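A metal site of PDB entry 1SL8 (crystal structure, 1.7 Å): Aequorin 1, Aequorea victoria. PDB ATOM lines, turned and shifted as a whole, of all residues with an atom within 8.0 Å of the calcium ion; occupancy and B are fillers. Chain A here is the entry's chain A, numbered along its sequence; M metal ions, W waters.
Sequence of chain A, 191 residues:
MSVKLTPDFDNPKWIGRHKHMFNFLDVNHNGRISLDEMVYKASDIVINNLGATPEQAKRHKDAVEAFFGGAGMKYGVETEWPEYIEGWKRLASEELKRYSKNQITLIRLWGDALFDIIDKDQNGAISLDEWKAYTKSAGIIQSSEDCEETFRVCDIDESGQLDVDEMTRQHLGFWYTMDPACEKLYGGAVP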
ATOM      1  N   PHE A  22       0.928  33.256 -17.541  1.00  0.00           N
ATOM      2  CA  PHE A  22       0.290  32.018 -17.992  1.00  0.00           C
ATOM      3  C   PHE A  22       0.336  31.036 -16.809  1.00  0.00           C
ATOM      4  O   PHE A  22      -0.690  30.464 -16.405  1.00  0.00           O
ATOM      5  CB  PHE A  22       1.066  31.533 -19.215  1.00  0.00           C
ATOM      6  CG  PHE A  22       0.661  30.173 -19.735  1.00  0.00           C
ATOM      7  CD1 PHE A  22      -0.155  30.083 -20.830  1.00  0.00           C
ATOM      8  CD2 PHE A  22       1.126  29.021 -19.131  1.00  0.00           C
ATOM      9  CE1 PHE A  22      -0.505  28.856 -21.378  1.00  0.00           C
ATOM     10  CE2 PHE A  22       0.750  27.759 -19.671  1.00  0.00           C
ATOM     11  CZ  PHE A  22      -0.037  27.683 -20.780  1.00  0.00           C
ATOM     12  N   ASN A  23       1.539  30.878 -16.243  1.00  0.00           N
ATOM     13  CA  ASN A  23       1.775  30.036 -15.049  1.00  0.00           C
ATOM     14  C   ASN A  23       0.900  30.442 -13.844  1.00  0.00           C
ATOM     15  O   ASN A  23       0.287  29.618 -13.147  1.00  0.00           O
ATOM     16  CB  ASN A  23       3.271  30.114 -14.714  1.00  0.00           C
ATOM     17  CG  ASN A  23       4.064  28.915 -15.224  1.00  0.00           C
ATOM     18  OD1 ASN A  23       4.029  28.578 -16.431  1.00  0.00           O
ATOM     19  ND2 ASN A  23       4.805  28.264 -14.312  1.00  0.00           N
ATOM     20  N   LEU A  25      -2.061  32.016 -13.920  1.00  0.00           N
ATOM     21  CA  LEU A  25      -3.479  31.749 -14.188  1.00  0.00           C
ATOM     22  C   LEU A  25      -3.818  30.286 -14.497  1.00  0.00           C
ATOM     23  O   LEU A  25      -5.004  29.929 -14.543  1.00  0.00           O
ATOM     24  CB  LEU A  25      -4.001  32.615 -15.350  1.00  0.00           C
ATOM     25  CG  LEU A  25      -3.751  34.137 -15.141  1.00  0.00           C
ATOM     26  CD1 LEU A  25      -4.017  34.878 -16.410  1.00  0.00           C
ATOM     27  CD2 LEU A  25      -4.596  34.673 -13.985  1.00  0.00           C
ATOM     28  N   ASP A  26      -2.782  29.474 -14.738  1.00  0.00           N
ATOM     29  CA  ASP A  26      -2.908  28.021 -15.017  1.00  0.00           C
ATOM     30  C   ASP A  26      -3.172  27.326 -13.673  1.00  0.00           C
ATOM     31  O   ASP A  26      -2.264  26.751 -13.069  1.00  0.00           O
ATOM     32  CB  ASP A  26      -1.605  27.514 -15.648  1.00  0.00           C
ATOM     33  CG  ASP A  26      -1.639  26.001 -15.970  1.00  0.00           C
ATOM     34  OD1 ASP A  26      -2.702  25.349 -15.904  1.00  0.00           O
ATOM     35  OD2 ASP A  26      -0.614  25.396 -16.327  1.00  0.00           O
ATOM     36  N   VAL A  27      -4.425  27.393 -13.249  1.00  0.00           N
ATOM     37  CA  VAL A  27      -4.870  27.029 -11.892  1.00  0.00           C
ATOM     38  C   VAL A  27      -4.433  25.591 -11.510  1.00  0.00           C
ATOM     39  O   VAL A  27      -4.063  25.347 -10.340  1.00  0.00           O
ATOM     40  CB  VAL A  27      -6.417  27.186 -11.771  1.00  0.00           C
ATOM     41  CG1 VAL A  27      -6.916  26.612 -10.474  1.00  0.00           C
ATOM     42  CG2 VAL A  27      -6.847  28.690 -11.801  1.00  0.00           C
ATOM     43  N   ASN A  28      -4.495  24.666 -12.471  1.00  0.00           N
ATOM     44  CA  ASN A  28      -4.145  23.257 -12.197  1.00  0.00           C
ATOM     45  C   ASN A  28      -2.707  22.901 -12.508  1.00  0.00           C
ATOM     46  O   ASN A  28      -2.292  21.734 -12.375  1.00  0.00           O
ATOM     47  CB  ASN A  28      -5.161  22.241 -12.802  1.00  0.00           C
ATOM     48  CG  ASN A  28      -5.119  22.156 -14.321  1.00  0.00           C
ATOM     49  OD1 ASN A  28      -4.317  22.811 -15.011  1.00  0.00           O
ATOM     50  ND2 ASN A  28      -6.005  21.363 -14.862  1.00  0.00           N
ATOM     51  N   HIS A  29      -1.938  23.916 -12.939  1.00  0.00           N
ATOM     52  CA  HIS A  29      -0.496  23.778 -13.136  1.00  0.00           C
ATOM     53  C   HIS A  29      -0.095  22.674 -14.126  1.00  0.00           C
ATOM     54  O   HIS A  29       0.957  22.067 -13.967  1.00  0.00           O
ATOM     55  CB  HIS A  29       0.231  23.572 -11.791  1.00  0.00           C
ATOM     56  CG  HIS A  29      -0.358  24.347 -10.642  1.00  0.00           C
ATOM     57  ND1 HIS A  29      -0.244  25.712 -10.527  1.00  0.00           N
ATOM     58  CD2 HIS A  29      -1.072  23.932  -9.562  1.00  0.00           C
ATOM     59  CE1 HIS A  29      -0.866  26.119  -9.435  1.00  0.00           C
ATOM     60  NE2 HIS A  29      -1.380  25.063  -8.834  1.00  0.00           N
ATOM     61  N   ASN A  30      -0.898  22.465 -15.183  1.00  0.00           N
ATOM     62  CA  ASN A  30      -0.636  21.415 -16.162  1.00  0.00           C
ATOM     63  C   ASN A  30       0.043  21.884 -17.445  1.00  0.00           C
ATOM     64  O   ASN A  30       0.393  21.063 -18.334  1.00  0.00           O
ATOM     65  CB  ASN A  30      -1.887  20.563 -16.428  1.00  0.00           C
ATOM     66  CG  ASN A  30      -2.855  21.210 -17.396  1.00  0.00           C
ATOM     67  OD1 ASN A  30      -2.931  22.452 -17.526  1.00  0.00           O
ATOM     68  ND2 ASN A  30      -3.638  20.381 -18.064  1.00  0.00           N
ATOM     69  N   GLY A  31       0.207  23.202 -17.560  1.00  0.00           N
ATOM     70  CA  GLY A  31       0.974  23.763 -18.675  1.00  0.00           C
ATOM     71  C   GLY A  31       0.122  24.000 -19.904  1.00  0.00           C
ATOM     72  O   GLY A  31       0.649  24.313 -20.964  1.00  0.00           O
ATOM     73  N   ARG A  32      -1.173  23.828 -19.741  1.00  0.00           N
ATOM     74  CA  ARG A  32      -2.189  24.209 -20.724  1.00  0.00           C
ATOM     75  C   ARG A  32      -3.214  25.119 -20.020  1.00  0.00           C
ATOM     76  O   ARG A  32      -3.393  25.031 -18.798  1.00  0.00           O
ATOM     77  CB  ARG A  32      -2.864  22.982 -21.351  1.00  0.00           C
ATOM     78  CG  ARG A  32      -1.822  21.889 -21.726  1.00  0.00           C
ATOM     79  CD  ARG A  32      -2.388  20.653 -22.443  1.00  0.00           C
ATOM     80  NE  ARG A  32      -1.330  19.866 -23.094  1.00  0.00           N
ATOM     81  CZ  ARG A  32      -1.409  19.356 -24.336  1.00  0.00           C
ATOM     82  NH1 ARG A  32      -2.484  19.580 -25.081  1.00  0.00           N
ATOM     83  NH2 ARG A  32      -0.401  18.631 -24.837  1.00  0.00           N
ATOM     84  N   ILE A  33      -3.840  26.039 -20.754  1.00  0.00           N
ATOM     85  CA  ILE A  33      -4.712  27.009 -20.092  1.00  0.00           C
ATOM     86  C   ILE A  33      -6.069  27.181 -20.776  1.00  0.00           C
ATOM     87  O   ILE A  33      -6.166  27.189 -21.993  1.00  0.00           O
ATOM     88  CB  ILE A  33      -3.981  28.378 -19.894  1.00  0.00           C
ATOM     89  CG1 ILE A  33      -4.665  29.212 -18.817  1.00  0.00           C
ATOM     90  CG2 ILE A  33      -3.913  29.138 -21.226  1.00  0.00           C
ATOM     91  CD1 ILE A  33      -3.816  30.376 -18.294  1.00  0.00           C
ATOM     92  N   SER A  34      -7.124  27.328 -19.967  1.00  0.00           N
ATOM     93  CA  SER A  34      -8.452  27.646 -20.496  1.00  0.00           C
ATOM     94  C   SER A  34      -8.964  29.022 -20.068  1.00  0.00           C
ATOM     95  O   SER A  34      -8.480  29.570 -19.105  1.00  0.00           O
ATOM     96  CB  SER A  34      -9.478  26.616 -20.012  1.00  0.00           C
ATOM     97  OG  SER A  34      -9.679  26.736 -18.603  1.00  0.00           O
ATOM     98  N   GLU A  37      -9.935  28.795 -16.494  1.00  0.00           N
ATOM     99  CA  GLU A  37      -8.868  29.019 -15.496  1.00  0.00           C
ATOM    100  C   GLU A  37      -8.625  30.525 -15.333  1.00  0.00           C
ATOM    101  O   GLU A  37      -8.621  31.040 -14.211  1.00  0.00           O
ATOM    102  CB  GLU A  37      -7.572  28.289 -15.862  1.00  0.00           C
ATOM    103  CG  GLU A  37      -7.682  26.766 -15.658  1.00  0.00           C
ATOM    104  CD  GLU A  37      -6.416  26.009 -15.988  1.00  0.00           C
ATOM    105  OE1 GLU A  37      -5.673  26.379 -16.952  1.00  0.00           O
ATOM    106  OE2 GLU A  37      -6.137  25.056 -15.244  1.00  0.00           O
ATOM    107  N   GLU A  78      -8.857  24.000 -23.860  1.00  0.00           N
ATOM    108  CA  GLU A  78      -7.496  24.147 -23.324  1.00  0.00           C
ATOM    109  C   GLU A  78      -6.574  24.640 -24.439  1.00  0.00           C
ATOM    110  O   GLU A  78      -6.636  24.141 -25.582  1.00  0.00           O
ATOM    111  CB  GLU A  78      -6.951  22.790 -22.834  1.00  0.00           C
ATOM    112  CG  GLU A  78      -7.216  22.447 -21.368  1.00  0.00           C
ATOM    113  CD  GLU A  78      -6.203  21.410 -20.840  1.00  0.00           C
ATOM    114  OE1 GLU A  78      -5.875  21.430 -19.625  1.00  0.00           O
ATOM    115  OE2 GLU A  78      -5.701  20.579 -21.655  1.00  0.00           O
ATOM    116  N   THR A  79      -5.705  25.586 -24.104  1.00  0.00           N
ATOM    117  CA  THR A  79      -4.826  26.183 -25.089  1.00  0.00           C
ATOM    118  C   THR A  79      -3.415  25.924 -24.656  1.00  0.00           C
ATOM    119  O   THR A  79      -3.083  26.101 -23.481  1.00  0.00           O
ATOM    120  CB  THR A  79      -5.090  27.726 -25.209  1.00  0.00           C
ATOM    121  OG1 THR A  79      -6.449  27.969 -25.594  1.00  0.00           O
ATOM    122  CG2 THR A  79      -4.259  28.325 -26.366  1.00  0.00           C
HETATM  123 CA    CA M   1      -4.365  24.332 -16.811  1.00  0.00          CA
HETATM  124  O   HOH W   1      -6.191  23.325 -17.751  1.00  0.00           O
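Water W1 lies within hydrogen-bond range of OE1 of Glu 78 (2.7 Å) and ND2 of Asn 28 (3.5 Å).
OD1 of Asp 26 is bound to the calcium ion, at 2.2 Å.
Water W1 binds the calcium ion, at 2.3 Å.
O of Arg 32 binds the calcium ion (2.3 Å).
The calcium ion is bound by the side-chain amide oxygen (OD1) of Asn 28 (2.4 Å).
The calcium ion is bound by OE1 of Glu 37.
OD1 of Asn 30 is bound to the calcium ion, at 2.5 Å.
The side-chain carboxylate (OE2) of Glu 37 is bound to the calcium ion, 2.5 Å away.
Five residues have an atom within 4 Å of the calcium ion: Asp 26, Asn 28, Asn 30, Arg 32 and Glu 37.
Along chain A the residues within 4 Å of the calcium ion span positions 26 to 37.
The nearest printed residue that does not touch the calcium ion is Ile 33 (4.2 Å).
O of Asp 26 sits at hydrogen-bond distance from ND1 of His 29, at 3.4 Å.
The side-chain carboxylate of Asp 26 sits at hydrogen-bond distance from the backbone NH of Gly 31, at 2.6 Å.
OG of Ser 34 is in hydrogen-bond range of N of Glu 37, 3.0 Å away.
OE1 of Glu 78 sits at hydrogen-bond distance from ND2 of Asn 30 (2.9 Å).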
